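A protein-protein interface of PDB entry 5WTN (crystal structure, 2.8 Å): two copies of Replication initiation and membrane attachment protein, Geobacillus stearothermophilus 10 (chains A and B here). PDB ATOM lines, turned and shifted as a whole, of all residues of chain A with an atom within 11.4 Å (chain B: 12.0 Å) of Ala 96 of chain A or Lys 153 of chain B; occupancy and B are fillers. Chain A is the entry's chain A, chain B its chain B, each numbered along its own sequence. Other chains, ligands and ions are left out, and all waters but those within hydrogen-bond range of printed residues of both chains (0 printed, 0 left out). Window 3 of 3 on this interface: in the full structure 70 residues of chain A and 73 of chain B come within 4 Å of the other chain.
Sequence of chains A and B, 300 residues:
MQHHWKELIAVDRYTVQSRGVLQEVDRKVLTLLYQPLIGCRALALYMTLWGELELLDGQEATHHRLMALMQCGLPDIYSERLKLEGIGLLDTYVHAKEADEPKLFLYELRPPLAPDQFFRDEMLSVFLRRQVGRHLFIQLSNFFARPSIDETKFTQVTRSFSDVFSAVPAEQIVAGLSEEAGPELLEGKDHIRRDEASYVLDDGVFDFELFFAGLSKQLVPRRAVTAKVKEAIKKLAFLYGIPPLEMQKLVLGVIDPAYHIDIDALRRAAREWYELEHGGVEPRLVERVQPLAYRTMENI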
ATOM      1  N   ASP A  12      11.272 -11.125   1.501  1.00  0.00           N
ATOM      2  CA  ASP A  12      10.729 -11.275   2.847  1.00  0.00           C
ATOM      3  C   ASP A  12      11.712 -12.091   3.687  1.00  0.00           C
ATOM      4  O   ASP A  12      12.454 -12.946   3.174  1.00  0.00           O
ATOM      5  CB  ASP A  12       9.357 -11.957   2.824  1.00  0.00           C
ATOM      6  CG  ASP A  12       8.239 -11.034   2.351  1.00  0.00           C
ATOM      7  OD1 ASP A  12       8.370  -9.805   2.562  1.00  0.00           O
ATOM      8  OD2 ASP A  12       7.225 -11.536   1.784  1.00  0.00           O
ATOM      9  N   ARG A  13      11.742 -11.837   4.991  1.00  0.00           N
ATOM     10  CA  ARG A  13      12.718 -12.500   5.856  1.00  0.00           C
ATOM     11  C   ARG A  13      12.101 -13.543   6.789  1.00  0.00           C
ATOM     12  O   ARG A  13      10.963 -13.395   7.231  1.00  0.00           O
ATOM     13  CB  ARG A  13      13.495 -11.465   6.675  1.00  0.00           C
ATOM     14  CG  ARG A  13      14.181 -10.399   5.836  1.00  0.00           C
ATOM     15  CD  ARG A  13      15.125  -9.557   6.678  1.00  0.00           C
ATOM     16  NE  ARG A  13      14.578  -9.283   8.004  1.00  0.00           N
ATOM     17  CZ  ARG A  13      13.753  -8.279   8.280  1.00  0.00           C
ATOM     18  NH1 ARG A  13      13.375  -7.446   7.319  1.00  0.00           N
ATOM     19  NH2 ARG A  13      13.304  -8.106   9.515  1.00  0.00           N
ATOM     20  N   THR A  15      12.947 -16.596  10.144  1.00  0.00           N
ATOM     21  CA  THR A  15      13.790 -17.300  11.084  1.00  0.00           C
ATOM     22  C   THR A  15      13.151 -18.665  11.299  1.00  0.00           C
ATOM     23  O   THR A  15      11.934 -18.804  11.153  1.00  0.00           O
ATOM     24  CB  THR A  15      13.900 -16.543  12.404  1.00  0.00           C
ATOM     25  OG1 THR A  15      14.677 -17.327  13.314  1.00  0.00           O
ATOM     26  CG2 THR A  15      12.527 -16.306  13.021  1.00  0.00           C
ATOM     27  N   GLN A  17      12.595 -21.680  14.130  1.00  0.00           N
ATOM     28  CA  GLN A  17      12.693 -21.997  15.559  1.00  0.00           C
ATOM     29  C   GLN A  17      11.961 -23.281  15.971  1.00  0.00           C
ATOM     30  O   GLN A  17      11.092 -23.795  15.241  1.00  0.00           O
ATOM     31  CB  GLN A  17      12.245 -20.783  16.392  1.00  0.00           C
ATOM     32  CG  GLN A  17      13.256 -19.650  16.299  1.00  0.00           C
ATOM     33  CD  GLN A  17      12.801 -18.351  16.895  1.00  0.00           C
ATOM     34  OE1 GLN A  17      12.772 -17.330  16.205  1.00  0.00           O
ATOM     35  NE2 GLN A  17      12.476 -18.356  18.183  1.00  0.00           N
ATOM     36  N   GLU A  60      18.553 -14.293  10.834  1.00  0.00           N
ATOM     37  CA  GLU A  60      17.654 -13.971   9.737  1.00  0.00           C
ATOM     38  C   GLU A  60      18.234 -14.361   8.383  1.00  0.00           C
ATOM     39  O   GLU A  60      19.450 -14.435   8.204  1.00  0.00           O
ATOM     40  CB  GLU A  60      17.311 -12.480   9.749  1.00  0.00           C
ATOM     41  CG  GLU A  60      16.818 -11.967  11.092  1.00  0.00           C
ATOM     42  CD  GLU A  60      15.931 -10.744  10.960  1.00  0.00           C
ATOM     43  OE1 GLU A  60      15.994 -10.073   9.907  1.00  0.00           O
ATOM     44  OE2 GLU A  60      15.172 -10.453  11.907  1.00  0.00           O
ATOM     45  N   THR A  92       3.416 -20.847  11.692  1.00  0.00           N
ATOM     46  CA  THR A  92       3.971 -19.667  11.051  1.00  0.00           C
ATOM     47  C   THR A  92       3.488 -18.403  11.725  1.00  0.00           C
ATOM     48  O   THR A  92       2.287 -18.206  11.912  1.00  0.00           O
ATOM     49  CB  THR A  92       3.651 -19.630   9.532  1.00  0.00           C
ATOM     50  OG1 THR A  92       4.213 -20.790   8.901  1.00  0.00           O
ATOM     51  CG2 THR A  92       4.229 -18.366   8.883  1.00  0.00           C
ATOM     52  N   TYR A  93       4.435 -17.547  12.090  1.00  0.00           N
ATOM     53  CA  TYR A  93       4.106 -16.261  12.683  1.00  0.00           C
ATOM     54  C   TYR A  93       4.644 -15.150  11.803  1.00  0.00           C
ATOM     55  O   TYR A  93       5.652 -15.326  11.117  1.00  0.00           O
ATOM     56  CB  TYR A  93       4.727 -16.141  14.077  1.00  0.00           C
ATOM     57  CG  TYR A  93       4.218 -17.129  15.106  1.00  0.00           C
ATOM     58  CD1 TYR A  93       3.200 -16.789  15.978  1.00  0.00           C
ATOM     59  CD2 TYR A  93       4.775 -18.404  15.218  1.00  0.00           C
ATOM     60  CE1 TYR A  93       2.745 -17.685  16.922  1.00  0.00           C
ATOM     61  CE2 TYR A  93       4.328 -19.301  16.163  1.00  0.00           C
ATOM     62  CZ  TYR A  93       3.315 -18.940  17.017  1.00  0.00           C
ATOM     63  OH  TYR A  93       2.864 -19.834  17.967  1.00  0.00           O
ATOM     64  N   VAL A  94       3.980 -13.999  11.840  1.00  0.00           N
ATOM     65  CA  VAL A  94       4.466 -12.822  11.114  1.00  0.00           C
ATOM     66  C   VAL A  94       4.743 -11.669  12.065  1.00  0.00           C
ATOM     67  O   VAL A  94       4.020 -11.454  13.035  1.00  0.00           O
ATOM     68  CB  VAL A  94       3.504 -12.382   9.963  1.00  0.00           C
ATOM     69  CG1 VAL A  94       2.316 -11.617  10.493  1.00  0.00           C
ATOM     70  CG2 VAL A  94       4.241 -11.554   8.936  1.00  0.00           C
ATOM     71  N   HIS A  95       5.818 -10.943  11.799  1.00  0.00           N
ATOM     72  CA  HIS A  95       6.156  -9.796  12.627  1.00  0.00           C
ATOM     73  C   HIS A  95       5.304  -8.610  12.239  1.00  0.00           C
ATOM     74  O   HIS A  95       5.112  -8.350  11.046  1.00  0.00           O
ATOM     75  CB  HIS A  95       7.627  -9.416  12.490  1.00  0.00           C
ATOM     76  CG  HIS A  95       8.079  -8.394  13.489  1.00  0.00           C
ATOM     77  ND1 HIS A  95       7.851  -7.045  13.330  1.00  0.00           N
ATOM     78  CD2 HIS A  95       8.747  -8.527  14.659  1.00  0.00           C
ATOM     79  CE1 HIS A  95       8.359  -6.390  14.358  1.00  0.00           C
ATOM     80  NE2 HIS A  95       8.908  -7.266  15.180  1.00  0.00           N
ATOM     81  N   ALA A  96       4.831  -7.887  13.258  1.00  0.00           N
ATOM     82  CA  ALA A  96       3.952  -6.729  13.084  1.00  0.00           C
ATOM     83  C   ALA A  96       4.604  -5.750  12.127  1.00  0.00           C
ATOM     84  O   ALA A  96       5.724  -5.295  12.367  1.00  0.00           O
ATOM     85  CB  ALA A  96       3.696  -6.056  14.430  1.00  0.00           C
ATOM     86  N   LYS A  97       3.896  -5.396  11.062  1.00  0.00           N
ATOM     87  CA  LYS A  97       4.572  -4.787   9.927  1.00  0.00           C
ATOM     88  C   LYS A  97       4.919  -3.321  10.162  1.00  0.00           C
ATOM     89  O   LYS A  97       4.042  -2.483  10.385  1.00  0.00           O
ATOM     90  CB  LYS A  97       3.743  -4.951   8.644  1.00  0.00           C
ATOM     91  CG  LYS A  97       3.593  -6.405   8.141  1.00  0.00           C
ATOM     92  CD  LYS A  97       2.306  -7.079   8.655  1.00  0.00           C
ATOM     93  CE  LYS A  97       1.992  -8.374   7.894  1.00  0.00           C
ATOM     94  NZ  LYS A  97       0.755  -9.058   8.395  1.00  0.00           N
ATOM     95  N   GLU A  98       6.220  -3.034  10.134  1.00  0.00           N
ATOM     96  CA  GLU A  98       6.738  -1.668  10.175  1.00  0.00           C
ATOM     97  C   GLU A  98       7.955  -1.539   9.235  1.00  0.00           C
ATOM     98  O   GLU A  98       8.917  -2.303   9.355  1.00  0.00           O
ATOM     99  CB  GLU A  98       7.093  -1.251  11.619  1.00  0.00           C
ATOM    100  CG  GLU A  98       5.887  -1.156  12.579  1.00  0.00           C
ATOM    101  CD  GLU A  98       6.234  -0.634  13.973  1.00  0.00           C
ATOM    102  OE1 GLU A  98       7.270   0.051  14.128  1.00  0.00           O
ATOM    103  OE2 GLU A  98       5.456  -0.908  14.917  1.00  0.00           O
ATOM    104  N   ALA A  99       7.912  -0.590   8.298  1.00  0.00           N
ATOM    105  CA  ALA A  99       6.724   0.219   8.065  1.00  0.00           C
ATOM    106  C   ALA A  99       5.795  -0.541   7.124  1.00  0.00           C
ATOM    107  O   ALA A  99       4.780  -1.095   7.556  1.00  0.00           O
ATOM    108  CB  ALA A  99       7.115   1.550   7.460  1.00  0.00           C
ATOM    109  N   ASP A 100       6.156  -0.562   5.841  1.00  0.00           N
ATOM    110  CA  ASP A 100       5.566  -1.488   4.867  1.00  0.00           C
ATOM    111  C   ASP A 100       6.665  -2.061   3.960  1.00  0.00           C
ATOM    112  O   ASP A 100       7.326  -1.320   3.213  1.00  0.00           O
ATOM    113  CB  ASP A 100       4.434  -0.832   4.056  1.00  0.00           C
ATOM    114  CG  ASP A 100       3.129  -0.713   4.852  1.00  0.00           C
ATOM    115  OD1 ASP A 100       2.826  -1.623   5.650  1.00  0.00           O
ATOM    116  OD2 ASP A 100       2.401   0.290   4.682  1.00  0.00           O
ATOM    117  N   GLU A 101       6.824  -3.386   4.042  1.00  0.00           N
ATOM    118  CA  GLU A 101       7.959  -4.144   3.489  1.00  0.00           C
ATOM    119  C   GLU A 101       9.261  -4.001   4.310  1.00  0.00           C
ATOM    120  O   GLU A 101       9.472  -2.998   5.016  1.00  0.00           O
ATOM    121  CB  GLU A 101       8.229  -3.803   2.001  1.00  0.00           C
ATOM    122  CG  GLU A 101       7.081  -4.079   1.016  1.00  0.00           C
ATOM    123  CD  GLU A 101       7.584  -4.376  -0.398  1.00  0.00           C
ATOM    124  OE1 GLU A 101       8.809  -4.263  -0.630  1.00  0.00           O
ATOM    125  OE2 GLU A 101       6.764  -4.733  -1.277  1.00  0.00           O
ATOM    126  N   PRO A 102      10.131  -5.025   4.231  1.00  0.00           N
ATOM    127  CA  PRO A 102       9.780  -6.421   3.932  1.00  0.00           C
ATOM    128  C   PRO A 102       9.323  -7.185   5.199  1.00  0.00           C
ATOM    129  O   PRO A 102       9.811  -6.909   6.309  1.00  0.00           O
ATOM    130  CB  PRO A 102      11.092  -7.007   3.376  1.00  0.00           C
ATOM    131  CG  PRO A 102      11.987  -5.816   3.120  1.00  0.00           C
ATOM    132  CD  PRO A 102      11.584  -4.819   4.164  1.00  0.00           C
ATOM    133  N   LYS A 103       8.443  -8.168   5.016  1.00  0.00           N
ATOM    134  CA  LYS A 103       7.904  -8.959   6.115  1.00  0.00           C
ATOM    135  C   LYS A 103       8.958  -9.817   6.845  1.00  0.00           C
ATOM    136  O   LYS A 103       9.970 -10.237   6.260  1.00  0.00           O
ATOM    137  CB  LYS A 103       6.800  -9.878   5.595  1.00  0.00           C
ATOM    138  CG  LYS A 103       5.511  -9.210   5.169  1.00  0.00           C
ATOM    139  CD  LYS A 103       4.628 -10.266   4.538  1.00  0.00           C
ATOM    140  CE  LYS A 103       3.183  -9.853   4.380  1.00  0.00           C
ATOM    141  NZ  LYS A 103       2.434 -11.009   3.797  1.00  0.00           N
ATOM    142  N   LEU A 104       8.710 -10.085   8.125  1.00  0.00           N
ATOM    143  CA  LEU A 104       9.554 -11.010   8.883  1.00  0.00           C
ATOM    144  C   LEU A 104       8.748 -12.223   9.390  1.00  0.00           C
ATOM    145  O   LEU A 104       7.896 -12.073  10.259  1.00  0.00           O
ATOM    146  CB  LEU A 104      10.215 -10.285  10.058  1.00  0.00           C
ATOM    147  CG  LEU A 104      11.017 -11.145  11.037  1.00  0.00           C
ATOM    148  CD1 LEU A 104      12.139 -11.880  10.326  1.00  0.00           C
ATOM    149  CD2 LEU A 104      11.559 -10.307  12.177  1.00  0.00           C
ATOM    150  N   PHE A 105       9.034 -13.409   8.858  1.00  0.00           N
ATOM    151  CA  PHE A 105       8.346 -14.637   9.273  1.00  0.00           C
ATOM    152  C   PHE A 105       9.079 -15.409  10.361  1.00  0.00           C
ATOM    153  O   PHE A 105      10.308 -15.461  10.372  1.00  0.00           O
ATOM    154  CB  PHE A 105       8.167 -15.572   8.084  1.00  0.00           C
ATOM    155  CG  PHE A 105       7.228 -15.055   7.069  1.00  0.00           C
ATOM    156  CD1 PHE A 105       5.870 -15.244   7.214  1.00  0.00           C
ATOM    157  CD2 PHE A 105       7.693 -14.347   5.970  1.00  0.00           C
ATOM    158  CE1 PHE A 105       4.982 -14.760   6.273  1.00  0.00           C
ATOM    159  CE2 PHE A 105       6.807 -13.849   5.024  1.00  0.00           C
ATOM    160  CZ  PHE A 105       5.449 -14.058   5.178  1.00  0.00           C
ATOM    161  N   LEU A 106       8.321 -16.009  11.271  1.00  0.00           N
ATOM    162  CA  LEU A 106       8.877 -16.966  12.214  1.00  0.00           C
ATOM    163  C   LEU A 106       8.360 -18.343  11.820  1.00  0.00           C
ATOM    164  O   LEU A 106       7.161 -18.594  11.840  1.00  0.00           O
ATOM    165  CB  LEU A 106       8.430 -16.618  13.629  1.00  0.00           C
ATOM    166  CG  LEU A 106       9.409 -16.886  14.774  1.00  0.00           C
ATOM    167  CD1 LEU A 106       8.924 -16.235  16.059  1.00  0.00           C
ATOM    168  CD2 LEU A 106       9.601 -18.379  14.949  1.00  0.00           C
ATOM    169  N   SER B 148      12.466 -18.087  23.737  1.00  0.00           N
ATOM    170  CA  SER B 148      11.017 -18.165  23.596  1.00  0.00           C
ATOM    171  C   SER B 148      10.499 -17.424  22.352  1.00  0.00           C
ATOM    172  O   SER B 148      11.272 -16.796  21.631  1.00  0.00           O
ATOM    173  CB  SER B 148      10.363 -17.585  24.849  1.00  0.00           C
ATOM    174  OG  SER B 148       8.963 -17.768  24.798  1.00  0.00           O
ATOM    175  N   ILE B 149       9.195 -17.494  22.097  1.00  0.00           N
ATOM    176  CA  ILE B 149       8.599 -16.710  21.015  1.00  0.00           C
ATOM    177  C   ILE B 149       7.901 -15.480  21.566  1.00  0.00           C
ATOM    178  O   ILE B 149       6.956 -15.605  22.359  1.00  0.00           O
ATOM    179  CB  ILE B 149       7.546 -17.507  20.242  1.00  0.00           C
ATOM    180  CG1 ILE B 149       8.205 -18.663  19.477  1.00  0.00           C
ATOM    181  CG2 ILE B 149       6.765 -16.583  19.307  1.00  0.00           C
ATOM    182  CD1 ILE B 149       7.246 -19.392  18.548  1.00  0.00           C
ATOM    183  N   ASP B 150       8.332 -14.297  21.128  1.00  0.00           N
ATOM    184  CA  ASP B 150       7.758 -13.073  21.666  1.00  0.00           C
ATOM    185  C   ASP B 150       6.408 -12.843  20.993  1.00  0.00           C
ATOM    186  O   ASP B 150       6.338 -12.512  19.806  1.00  0.00           O
ATOM    187  CB  ASP B 150       8.700 -11.912  21.363  1.00  0.00           C
ATOM    188  CG  ASP B 150       8.376 -10.664  22.158  1.00  0.00           C
ATOM    189  OD1 ASP B 150       7.213 -10.514  22.604  1.00  0.00           O
ATOM    190  OD2 ASP B 150       9.299  -9.831  22.325  1.00  0.00           O
ATOM    191  N   GLU B 151       5.343 -12.948  21.782  1.00  0.00           N
ATOM    192  CA  GLU B 151       3.987 -12.916  21.254  1.00  0.00           C
ATOM    193  C   GLU B 151       3.526 -11.469  21.077  1.00  0.00           C
ATOM    194  O   GLU B 151       2.525 -11.199  20.416  1.00  0.00           O
ATOM    195  CB  GLU B 151       3.029 -13.681  22.179  1.00  0.00           C
ATOM    196  CG  GLU B 151       3.019 -13.172  23.641  1.00  0.00           C
ATOM    197  CD  GLU B 151       1.833 -13.680  24.474  1.00  0.00           C
ATOM    198  OE1 GLU B 151       0.737 -13.066  24.406  1.00  0.00           O
ATOM    199  OE2 GLU B 151       2.008 -14.677  25.214  1.00  0.00           O
ATOM    200  N   THR B 152       4.263 -10.540  21.675  1.00  0.00           N
ATOM    201  CA  THR B 152       3.957  -9.125  21.534  1.00  0.00           C
ATOM    202  C   THR B 152       4.296  -8.669  20.121  1.00  0.00           C
ATOM    203  O   THR B 152       3.571  -7.879  19.519  1.00  0.00           O
ATOM    204  CB  THR B 152       4.746  -8.270  22.546  1.00  0.00           C
ATOM    205  OG1 THR B 152       6.138  -8.260  22.196  1.00  0.00           O
ATOM    206  CG2 THR B 152       4.585  -8.812  23.949  1.00  0.00           C
ATOM    207  N   LYS B 153       5.421  -9.158  19.612  1.00  0.00           N
ATOM    208  CA  LYS B 153       5.916  -8.779  18.300  1.00  0.00           C
ATOM    209  C   LYS B 153       5.500  -9.717  17.156  1.00  0.00           C
ATOM    210  O   LYS B 153       5.678  -9.377  15.985  1.00  0.00           O
ATOM    211  CB  LYS B 153       7.442  -8.677  18.352  1.00  0.00           C
ATOM    212  CG  LYS B 153       7.976  -7.791  19.484  1.00  0.00           C
ATOM    213  CD  LYS B 153       9.504  -7.597  19.392  1.00  0.00           C
ATOM    214  CE  LYS B 153       9.982  -6.351  20.165  1.00  0.00           C
ATOM    215  NZ  LYS B 153       9.900  -6.496  21.654  1.00  0.00           N
ATOM    216  N   PHE B 154       4.947 -10.885  17.478  1.00  0.00           N
ATOM    217  CA  PHE B 154       4.601 -11.866  16.440  1.00  0.00           C
ATOM    218  C   PHE B 154       3.176 -12.363  16.543  1.00  0.00           C
ATOM    219  O   PHE B 154       2.650 -12.583  17.638  1.00  0.00           O
ATOM    220  CB  PHE B 154       5.515 -13.077  16.504  1.00  0.00           C
ATOM    221  CG  PHE B 154       6.895 -12.825  15.989  1.00  0.00           C
ATOM    222  CD1 PHE B 154       7.197 -13.031  14.651  1.00  0.00           C
ATOM    223  CD2 PHE B 154       7.906 -12.401  16.845  1.00  0.00           C
ATOM    224  CE1 PHE B 154       8.482 -12.807  14.167  1.00  0.00           C
ATOM    225  CE2 PHE B 154       9.191 -12.179  16.369  1.00  0.00           C
ATOM    226  CZ  PHE B 154       9.478 -12.379  15.032  1.00  0.00           C
ATOM    227  N   THR B 155       2.561 -12.578  15.391  1.00  0.00           N
ATOM    228  CA  THR B 155       1.186 -13.034  15.363  1.00  0.00           C
ATOM    229  C   THR B 155       1.062 -14.199  14.384  1.00  0.00           C
ATOM    230  O   THR B 155       1.721 -14.224  13.331  1.00  0.00           O
ATOM    231  CB  THR B 155       0.217 -11.880  15.035  1.00  0.00           C
ATOM    232  OG1 THR B 155      -1.084 -12.405  14.745  1.00  0.00           O
ATOM    233  CG2 THR B 155       0.724 -11.070  13.846  1.00  0.00           C
ATOM    234  N   GLN B 156       0.243 -15.179  14.759  1.00  0.00           N
ATOM    235  CA  GLN B 156       0.191 -16.443  14.047  1.00  0.00           C
ATOM    236  C   GLN B 156      -0.655 -16.329  12.788  1.00  0.00           C
ATOM    237  O   GLN B 156      -1.807 -15.890  12.837  1.00  0.00           O
ATOM    238  CB  GLN B 156      -0.328 -17.541  14.973  1.00  0.00           C
ATOM    239  CG  GLN B 156      -0.336 -18.935  14.355  1.00  0.00           C
ATOM    240  CD  GLN B 156      -0.141 -20.046  15.388  1.00  0.00           C
ATOM    241  OE1 GLN B 156      -0.166 -19.799  16.600  1.00  0.00           O
ATOM    242  NE2 GLN B 156       0.051 -21.278  14.908  1.00  0.00           N
ATOM    243  N   VAL B 157      -0.025 -16.618  11.651  1.00  0.00           N
ATOM    244  CA  VAL B 157      -0.703 -16.729  10.362  1.00  0.00           C
ATOM    245  C   VAL B 157      -0.902 -18.168   9.909  1.00  0.00           C
ATOM    246  O   VAL B 157      -1.223 -18.407   8.736  1.00  0.00           O
ATOM    247  CB  VAL B 157      -0.008 -15.906   9.265  1.00  0.00           C
ATOM    248  CG1 VAL B 157       0.017 -14.422   9.652  1.00  0.00           C
ATOM    249  CG2 VAL B 157       1.388 -16.438   9.030  1.00  0.00           C
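O of Thr 92 of chain A lies within hydrogen-bond range of N of Val 157 of chain B.
OH of Tyr 93 of chain A is in hydrogen-bond range of OE1 of Gln 156 of chain B, 3.3 Å away.
O of Thr 155 of chain B sits at hydrogen-bond distance from N of Val 94 of chain A (2.7 Å).
N of Ala 96 of chain A is in hydrogen-bond range of O of Lys 153 of chain B.
The side-chain amide oxygen (OE1) of Gln 17 of chain A sits close to the side-chain hydroxyl (OG1) of Thr 15 of chain A.
The backbone carbonyl oxygen (O) of Tyr 93 of chain A is in hydrogen-bond range of the backbone NH (N) of Leu 106 of chain A (2.8 Å).
O of Leu 104 of chain A lies within hydrogen-bond range of N of His 95 of chain A, at 2.8 Å.
The side-chain carboxylate (OD2) of Asp 150 of chain B lies within salt-bridge range of the side-chain amino group (NZ) of Lys 153 of chain B (3.5 Å).
Among the printed residues, pairs that only touch across the chains: Tyr 93 of chain A with Thr 155 of chain B (3.2 Å), His 95 of chain A with Lys 153 of chain B (3.4 Å), Thr 92 of chain A with Gln 156 of chain B (3.5 Å), Val 94 of chain A with Phe 154 of chain B (3.5 Å), Val 94 of chain A with Val 157 of chain B (3.7 Å), Tyr 93 of chain A with Ile 149 of chain B (3.8 Å), His 95 of chain A with Phe 154 of chain B (3.8 Å), Leu 106 of chain A with Phe 154 of chain B (3.8 Å), Leu 106 of chain A with Ile 149 of chain B (3.9 Å), Val 94 of chain A with Lys 153 of chain B (3.97 Å), Gln 17 of chain A with Ser 148 of chain B (3.97 Å) and Tyr 93 of chain A with Phe 154 of chain B (3.99 Å).
Lys 153 of chain B touches just these residues of chain A: Val 94 (3.97 Å), His 95 (3.4 Å) and Ala 96 (3.2 Å).
Val 94 of chain A touches just these residues of chain B: Lys 153 (3.97 Å), Phe 154 (3.5 Å), Thr 155 (2.7 Å) and Val 157 (3.7 Å).
No residue of chain B comes within 4 Å of Lys 97 of chain A.
No residue of chain B comes within 4 Å of Glu 98 of chain A.
No residue of chain A comes within 4 Å of Thr 152 of chain B.
Of the printed residues of chain A, Ser 148 of chain B touches Gln 17.
Of the printed residues of chain A, Val 157 of chain B touches Thr 92 and Val 94.
Of the printed residues of chain B, Gln 17 of chain A touches Ser 148 (3.97 Å).
Printed residues of chain B within 4 Å of Leu 106 of chain A: Ile 149 (3.9 Å) and Phe 154 (3.8 Å).
Of the printed residues of chain A, Ile 149 of chain B touches Tyr 93 (3.8 Å) and Leu 106 (3.9 Å).
The nearest residue of chain A that does not touch Lys 153 of chain B is Lys 97 of chain A (6.6 Å).
Of the 10 printed residues of chain B, 7 touch a printed residue of chain A.
Printed residues of chain B that touch a printed residue of chain A: Ser 148, Ile 149, Lys 153, Phe 154, Thr 155, Gln 156 and Val 157.
Hydrophobic or aromatic side chains of chain B within 4 Å of the printed part of chain A: Ile 149, Phe 154 and Val 157.
Of the 20 printed residues of chain A, 7 touch a printed residue of chain B.
Hydrophobic or aromatic side chains of chain A within 4 Å of the printed part of chain B: Tyr 93, Val 94, His 95 and Leu 106.
Among the printed residues, 16 pairs touch across the chains.
No position is printed for both chains.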
